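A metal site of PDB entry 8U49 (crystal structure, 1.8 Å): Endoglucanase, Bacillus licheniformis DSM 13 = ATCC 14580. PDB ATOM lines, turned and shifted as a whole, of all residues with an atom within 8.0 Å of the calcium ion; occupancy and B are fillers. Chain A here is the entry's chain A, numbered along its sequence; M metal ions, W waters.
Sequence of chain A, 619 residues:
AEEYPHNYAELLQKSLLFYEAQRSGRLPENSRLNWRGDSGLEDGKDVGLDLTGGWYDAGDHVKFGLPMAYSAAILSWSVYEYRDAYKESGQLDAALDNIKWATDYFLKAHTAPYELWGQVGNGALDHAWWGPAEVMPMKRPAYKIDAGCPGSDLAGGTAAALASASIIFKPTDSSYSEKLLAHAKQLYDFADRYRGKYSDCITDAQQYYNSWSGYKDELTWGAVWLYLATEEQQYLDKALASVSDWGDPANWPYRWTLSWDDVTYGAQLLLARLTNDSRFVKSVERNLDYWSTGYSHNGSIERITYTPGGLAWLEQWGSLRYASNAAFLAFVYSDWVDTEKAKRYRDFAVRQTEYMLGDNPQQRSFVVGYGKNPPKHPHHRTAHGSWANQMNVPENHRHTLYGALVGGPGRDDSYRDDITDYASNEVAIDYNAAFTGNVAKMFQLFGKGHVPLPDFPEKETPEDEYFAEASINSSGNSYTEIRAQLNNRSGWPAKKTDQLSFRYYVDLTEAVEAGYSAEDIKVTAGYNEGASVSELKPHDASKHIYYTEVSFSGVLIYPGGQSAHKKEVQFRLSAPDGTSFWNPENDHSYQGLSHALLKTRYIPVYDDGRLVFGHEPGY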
ATOM      1  N   LEU A  66     -33.283  16.697 -21.374  1.00  0.00           N
ATOM      2  CA  LEU A  66     -31.947  16.407 -20.828  1.00  0.00           C
ATOM      3  C   LEU A  66     -31.908  16.640 -19.328  1.00  0.00           C
ATOM      4  O   LEU A  66     -31.534  15.708 -18.591  1.00  0.00           O
ATOM      5  CB  LEU A  66     -30.875  17.208 -21.570  1.00  0.00           C
ATOM      6  CG  LEU A  66     -29.457  16.865 -21.112  1.00  0.00           C
ATOM      7  CD1 LEU A  66     -29.104  15.420 -21.492  1.00  0.00           C
ATOM      8  CD2 LEU A  66     -28.480  17.852 -21.711  1.00  0.00           C
ATOM      9  N   SER A 152     -26.781  11.677 -28.413  1.00  0.00           N
ATOM     10  CA  SER A 152     -26.179  10.697 -27.514  1.00  0.00           C
ATOM     11  C   SER A 152     -26.203  11.177 -26.072  1.00  0.00           C
ATOM     12  O   SER A 152     -26.227  10.351 -25.151  1.00  0.00           O
ATOM     13  CB  SER A 152     -24.734  10.394 -27.931  1.00  0.00           C
ATOM     14  OG  SER A 152     -24.656   9.999 -29.285  1.00  0.00           O
ATOM     15  N   ASP A 153     -26.195  12.495 -25.861  1.00  0.00           N
ATOM     16  CA  ASP A 153     -26.302  13.017 -24.512  1.00  0.00           C
ATOM     17  C   ASP A 153     -27.688  12.777 -23.938  1.00  0.00           C
ATOM     18  O   ASP A 153     -27.835  12.219 -22.845  1.00  0.00           O
ATOM     19  CB  ASP A 153     -25.952  14.511 -24.477  1.00  0.00           C
ATOM     20  CG  ASP A 153     -26.315  15.252 -25.768  1.00  0.00           C
ATOM     21  OD1 ASP A 153     -27.235  14.808 -26.502  1.00  0.00           O
ATOM     22  OD2 ASP A 153     -25.656  16.271 -26.061  1.00  0.00           O
ATOM     23  N   LEU A 154     -28.728  13.189 -24.675  1.00  0.00           N
ATOM     24  CA  LEU A 154     -30.107  12.943 -24.246  1.00  0.00           C
ATOM     25  C   LEU A 154     -30.379  11.447 -24.117  1.00  0.00           C
ATOM     26  O   LEU A 154     -30.940  10.986 -23.110  1.00  0.00           O
ATOM     27  CB  LEU A 154     -31.093  13.587 -25.228  1.00  0.00           C
ATOM     28  CG  LEU A 154     -32.574  13.352 -24.930  1.00  0.00           C
ATOM     29  CD1 LEU A 154     -32.943  13.902 -23.552  1.00  0.00           C
ATOM     30  CD2 LEU A 154     -33.468  13.979 -25.993  1.00  0.00           C
ATOM     31  N   LYS A 197     -24.781  15.649 -30.593  1.00  0.00           N
ATOM     32  CA  LYS A 197     -25.393  16.383 -29.506  1.00  0.00           C
ATOM     33  C   LYS A 197     -26.875  16.604 -29.804  1.00  0.00           C
ATOM     34  O   LYS A 197     -27.228  17.015 -30.914  1.00  0.00           O
ATOM     35  CB  LYS A 197     -24.703  17.737 -29.296  1.00  0.00           C
ATOM     36  CG  LYS A 197     -23.206  17.634 -29.002  1.00  0.00           C
ATOM     37  CD  LYS A 197     -22.598  19.011 -28.756  1.00  0.00           C
ATOM     38  CE  LYS A 197     -22.452  19.799 -30.042  1.00  0.00           C
ATOM     39  NZ  LYS A 197     -21.914  21.163 -29.794  1.00  0.00           N
ATOM     40  N   ASN A 210     -28.411  23.974 -23.633  1.00  0.00           N
ATOM     41  CA  ASN A 210     -27.423  23.640 -24.645  1.00  0.00           C
ATOM     42  C   ASN A 210     -26.467  22.555 -24.133  1.00  0.00           C
ATOM     43  O   ASN A 210     -26.067  22.554 -22.968  1.00  0.00           O
ATOM     44  CB  ASN A 210     -26.634  24.894 -25.029  1.00  0.00           C
ATOM     45  CG  ASN A 210     -25.805  24.696 -26.267  1.00  0.00           C
ATOM     46  OD1 ASN A 210     -26.222  24.015 -27.195  1.00  0.00           O
ATOM     47  ND2 ASN A 210     -24.604  25.287 -26.287  1.00  0.00           N
ATOM     48  N   SER A 211     -26.081  21.646 -25.023  1.00  0.00           N
ATOM     49  CA  SER A 211     -25.122  20.606 -24.659  1.00  0.00           C
ATOM     50  C   SER A 211     -23.712  21.199 -24.684  1.00  0.00           C
ATOM     51  O   SER A 211     -22.923  20.983 -25.601  1.00  0.00           O
ATOM     52  CB  SER A 211     -25.250  19.400 -25.569  1.00  0.00           C
ATOM     53  OG  SER A 211     -24.425  18.339 -25.107  1.00  0.00           O
ATOM     54  N   TRP A 212     -23.423  22.010 -23.664  1.00  0.00           N
ATOM     55  CA  TRP A 212     -22.113  22.673 -23.600  1.00  0.00           C
ATOM     56  C   TRP A 212     -20.987  21.647 -23.542  1.00  0.00           C
ATOM     57  O   TRP A 212     -19.974  21.790 -24.224  1.00  0.00           O
ATOM     58  CB  TRP A 212     -22.041  23.619 -22.402  1.00  0.00           C
ATOM     59  CG  TRP A 212     -23.124  24.662 -22.364  1.00  0.00           C
ATOM     60  CD1 TRP A 212     -24.256  24.652 -21.588  1.00  0.00           C
ATOM     61  CD2 TRP A 212     -23.177  25.880 -23.130  1.00  0.00           C
ATOM     62  NE1 TRP A 212     -24.998  25.784 -21.823  1.00  0.00           N
ATOM     63  CE2 TRP A 212     -24.358  26.553 -22.768  1.00  0.00           C
ATOM     64  CE3 TRP A 212     -22.330  26.457 -24.087  1.00  0.00           C
ATOM     65  CZ2 TRP A 212     -24.724  27.771 -23.330  1.00  0.00           C
ATOM     66  CZ3 TRP A 212     -22.686  27.678 -24.649  1.00  0.00           C
ATOM     67  CH2 TRP A 212     -23.878  28.317 -24.258  1.00  0.00           C
ATOM     68  N   SER A 213     -21.162  20.585 -22.758  1.00  0.00           N
ATOM     69  CA  SER A 213     -20.084  19.623 -22.553  1.00  0.00           C
ATOM     70  C   SER A 213     -20.008  18.560 -23.640  1.00  0.00           C
ATOM     71  O   SER A 213     -19.035  17.796 -23.654  1.00  0.00           O
ATOM     72  CB  SER A 213     -20.237  18.950 -21.200  1.00  0.00           C
ATOM     73  OG  SER A 213     -21.449  18.225 -21.150  1.00  0.00           O
ATOM     74  N   GLY A 214     -20.988  18.466 -24.537  1.00  0.00           N
ATOM     75  CA  GLY A 214     -20.988  17.358 -25.476  1.00  0.00           C
ATOM     76  C   GLY A 214     -21.567  16.100 -24.833  1.00  0.00           C
ATOM     77  O   GLY A 214     -22.217  16.153 -23.796  1.00  0.00           O
ATOM     78  N   TYR A 215     -21.307  14.954 -25.470  1.00  0.00           N
ATOM     79  CA  TYR A 215     -21.953  13.710 -25.064  1.00  0.00           C
ATOM     80  C   TYR A 215     -20.986  12.627 -24.587  1.00  0.00           C
ATOM     81  O   TYR A 215     -21.442  11.548 -24.205  1.00  0.00           O
ATOM     82  CB  TYR A 215     -22.806  13.144 -26.215  1.00  0.00           C
ATOM     83  CG  TYR A 215     -22.046  12.941 -27.504  1.00  0.00           C
ATOM     84  CD1 TYR A 215     -21.207  11.856 -27.685  1.00  0.00           C
ATOM     85  CD2 TYR A 215     -22.163  13.863 -28.538  1.00  0.00           C
ATOM     86  CE1 TYR A 215     -20.504  11.683 -28.856  1.00  0.00           C
ATOM     87  CE2 TYR A 215     -21.452  13.698 -29.717  1.00  0.00           C
ATOM     88  CZ  TYR A 215     -20.633  12.608 -29.863  1.00  0.00           C
ATOM     89  OH  TYR A 215     -19.931  12.441 -31.043  1.00  0.00           O
ATOM     90  N   LYS A 216     -19.681  12.885 -24.605  1.00  0.00           N
ATOM     91  CA  LYS A 216     -18.759  11.850 -24.152  1.00  0.00           C
ATOM     92  C   LYS A 216     -19.022  11.478 -22.693  1.00  0.00           C
ATOM     93  O   LYS A 216     -18.834  10.320 -22.304  1.00  0.00           O
ATOM     94  CB  LYS A 216     -17.312  12.311 -24.339  1.00  0.00           C
ATOM     95  CG  LYS A 216     -16.880  12.408 -25.795  1.00  0.00           C
ATOM     96  CD  LYS A 216     -15.461  13.018 -25.904  1.00  0.00           C
ATOM     97  CE  LYS A 216     -14.988  13.118 -27.363  1.00  0.00           C
ATOM     98  NZ  LYS A 216     -13.498  13.237 -27.508  1.00  0.00           N
ATOM     99  N   ASP A 217     -19.481  12.430 -21.873  1.00  0.00           N
ATOM    100  CA  ASP A 217     -19.744  12.101 -20.481  1.00  0.00           C
ATOM    101  C   ASP A 217     -20.977  11.199 -20.356  1.00  0.00           C
ATOM    102  O   ASP A 217     -20.966  10.248 -19.569  1.00  0.00           O
ATOM    103  CB  ASP A 217     -19.882  13.364 -19.631  1.00  0.00           C
ATOM    104  CG  ASP A 217     -20.762  14.424 -20.260  1.00  0.00           C
ATOM    105  OD1 ASP A 217     -20.535  14.769 -21.440  1.00  0.00           O
ATOM    106  OD2 ASP A 217     -21.679  14.912 -19.576  1.00  0.00           O
ATOM    107  N   GLU A 218     -22.038  11.480 -21.131  1.00  0.00           N
ATOM    108  CA  GLU A 218     -23.242  10.654 -21.013  1.00  0.00           C
ATOM    109  C   GLU A 218     -23.009   9.243 -21.532  1.00  0.00           C
ATOM    110  O   GLU A 218     -23.647   8.296 -21.049  1.00  0.00           O
ATOM    111  CB  GLU A 218     -24.426  11.294 -21.762  1.00  0.00           C
ATOM    112  CG  GLU A 218     -25.076  12.498 -21.038  1.00  0.00           C
ATOM    113  CD  GLU A 218     -24.342  13.811 -21.289  1.00  0.00           C
ATOM    114  OE1 GLU A 218     -23.363  13.805 -22.064  1.00  0.00           O
ATOM    115  OE2 GLU A 218     -24.743  14.845 -20.708  1.00  0.00           O
ATOM    116  N   LEU A 219     -22.118   9.078 -22.515  1.00  0.00           N
ATOM    117  CA  LEU A 219     -21.820   7.721 -22.988  1.00  0.00           C
ATOM    118  C   LEU A 219     -21.207   6.879 -21.871  1.00  0.00           C
ATOM    119  O   LEU A 219     -21.549   5.703 -21.724  1.00  0.00           O
ATOM    120  CB  LEU A 219     -20.906   7.788 -24.213  1.00  0.00           C
ATOM    121  CG  LEU A 219     -21.592   8.284 -25.484  1.00  0.00           C
ATOM    122  CD1 LEU A 219     -20.614   8.339 -26.654  1.00  0.00           C
ATOM    123  CD2 LEU A 219     -22.800   7.396 -25.819  1.00  0.00           C
ATOM    124  N   SER A 259     -23.725  18.128 -13.054  1.00  0.00           N
ATOM    125  CA  SER A 259     -24.898  18.912 -13.419  1.00  0.00           C
ATOM    126  C   SER A 259     -25.662  18.193 -14.531  1.00  0.00           C
ATOM    127  O   SER A 259     -25.204  17.172 -15.065  1.00  0.00           O
ATOM    128  CB  SER A 259     -24.525  20.331 -13.861  1.00  0.00           C
ATOM    129  OG  SER A 259     -24.003  20.324 -15.179  1.00  0.00           O
ATOM    130  N   TRP A 260     -26.817  18.753 -14.900  1.00  0.00           N
ATOM    131  CA  TRP A 260     -27.609  18.222 -16.016  1.00  0.00           C
ATOM    132  C   TRP A 260     -26.805  18.178 -17.300  1.00  0.00           C
ATOM    133  O   TRP A 260     -27.114  17.379 -18.195  1.00  0.00           O
ATOM    134  CB  TRP A 260     -28.871  19.069 -16.216  1.00  0.00           C
ATOM    135  CG  TRP A 260     -28.543  20.511 -16.522  1.00  0.00           C
ATOM    136  CD1 TRP A 260     -28.486  21.546 -15.632  1.00  0.00           C
ATOM    137  CD2 TRP A 260     -28.196  21.057 -17.801  1.00  0.00           C
ATOM    138  NE1 TRP A 260     -28.128  22.707 -16.279  1.00  0.00           N
ATOM    139  CE2 TRP A 260     -27.933  22.437 -17.611  1.00  0.00           C
ATOM    140  CE3 TRP A 260     -28.087  20.521 -19.088  1.00  0.00           C
ATOM    141  CZ2 TRP A 260     -27.584  23.282 -18.660  1.00  0.00           C
ATOM    142  CZ3 TRP A 260     -27.716  21.358 -20.132  1.00  0.00           C
ATOM    143  CH2 TRP A 260     -27.461  22.724 -19.903  1.00  0.00           C
ATOM    144  N   ASP A 261     -25.800  19.041 -17.428  1.00  0.00           N
ATOM    145  CA  ASP A 261     -25.003  19.145 -18.639  1.00  0.00           C
ATOM    146  C   ASP A 261     -23.787  18.233 -18.597  1.00  0.00           C
ATOM    147  O   ASP A 261     -23.493  17.532 -19.575  1.00  0.00           O
ATOM    148  CB  ASP A 261     -24.554  20.589 -18.844  1.00  0.00           C
ATOM    149  CG  ASP A 261     -23.602  20.765 -20.046  1.00  0.00           C
ATOM    150  OD1 ASP A 261     -23.687  20.002 -21.032  1.00  0.00           O
ATOM    151  OD2 ASP A 261     -22.770  21.687 -19.988  1.00  0.00           O
ATOM    152  N   ASP A 262     -23.061  18.235 -17.475  1.00  0.00           N
ATOM    153  CA  ASP A 262     -21.808  17.500 -17.382  1.00  0.00           C
ATOM    154  C   ASP A 262     -21.917  16.424 -16.303  1.00  0.00           C
ATOM    155  O   ASP A 262     -21.856  16.733 -15.111  1.00  0.00           O
ATOM    156  CB  ASP A 262     -20.647  18.442 -17.080  1.00  0.00           C
ATOM    157  CG  ASP A 262     -19.310  17.795 -17.378  1.00  0.00           C
ATOM    158  OD1 ASP A 262     -19.253  16.549 -17.453  1.00  0.00           O
ATOM    159  OD2 ASP A 262     -18.320  18.543 -17.547  1.00  0.00           O
ATOM    160  N   VAL A 263     -22.074  15.173 -16.723  1.00  0.00           N
ATOM    161  CA  VAL A 263     -22.146  14.062 -15.784  1.00  0.00           C
ATOM    162  C   VAL A 263     -20.805  13.345 -15.671  1.00  0.00           C
ATOM    163  O   VAL A 263     -20.738  12.218 -15.143  1.00  0.00           O
ATOM    164  CB  VAL A 263     -23.284  13.090 -16.143  1.00  0.00           C
ATOM    165  CG1 VAL A 263     -24.619  13.776 -15.926  1.00  0.00           C
ATOM    166  CG2 VAL A 263     -23.153  12.605 -17.578  1.00  0.00           C
ATOM    167  N   THR A 264     -19.715  13.954 -16.154  1.00  0.00           N
ATOM    168  CA  THR A 264     -18.390  13.375 -15.958  1.00  0.00           C
ATOM    169  C   THR A 264     -18.162  13.045 -14.494  1.00  0.00           C
ATOM    170  O   THR A 264     -17.670  11.958 -14.153  1.00  0.00           O
ATOM    171  CB  THR A 264     -17.302  14.354 -16.425  1.00  0.00           C
ATOM    172  OG1 THR A 264     -17.516  14.729 -17.795  1.00  0.00           O
ATOM    173  CG2 THR A 264     -15.914  13.720 -16.282  1.00  0.00           C
HETATM  174 CA    CA M   1     -22.741  16.154 -21.423  1.00  0.00          CA
HETATM  175  O   HOH W   1     -24.363  17.747 -22.308  1.00  0.00           O
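Five residues have an atom within 4 Å of the calcium ion: Ser 213, Gly 214, Asp 217, Glu 218 and Asp 261.
The nearest printed residue that does not touch the calcium ion is Asp 262 (4.4 Å).
Water W1 bridges OD1 of Asp 261 (2.7 Å) and OG of Ser 211 (2.9 Å).
The calcium ion is bound by O of Asp 261 (2.4 Å).
The backbone carbonyl oxygen (O) of Gly 214 binds the calcium ion (2.4 Å).
Water W1 is bound to the calcium ion (2.4 Å).
OG of Ser 213 is bound to the calcium ion (2.5 Å).
The calcium ion is bound by the side-chain carboxylate (OD2) of Asp 217, 2.5 Å away.
The calcium ion is bound by the side-chain carboxylate (OE2) of Glu 218 (2.5 Å).
OE1 of Glu 218 binds the calcium ion, at 2.5 Å.
OD1 of Asp 217 binds the calcium ion, at 2.6 Å.
The side-chain hydroxyl of Ser 211 sits at hydrogen-bond distance from the backbone NH of Gly 214, at 3.5 Å.
The side-chain carboxylate (OD2) of Asp 217 lies close to the backbone NH (N) of Val 263 (2.9 Å).
The backbone NH (N) of Asp 261 lies close to the side-chain hydroxyl (OG) of Ser 259 (3.2 Å).
N of Trp 212 sits at hydrogen-bond distance from OD1 of Asp 261 (3.3 Å).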
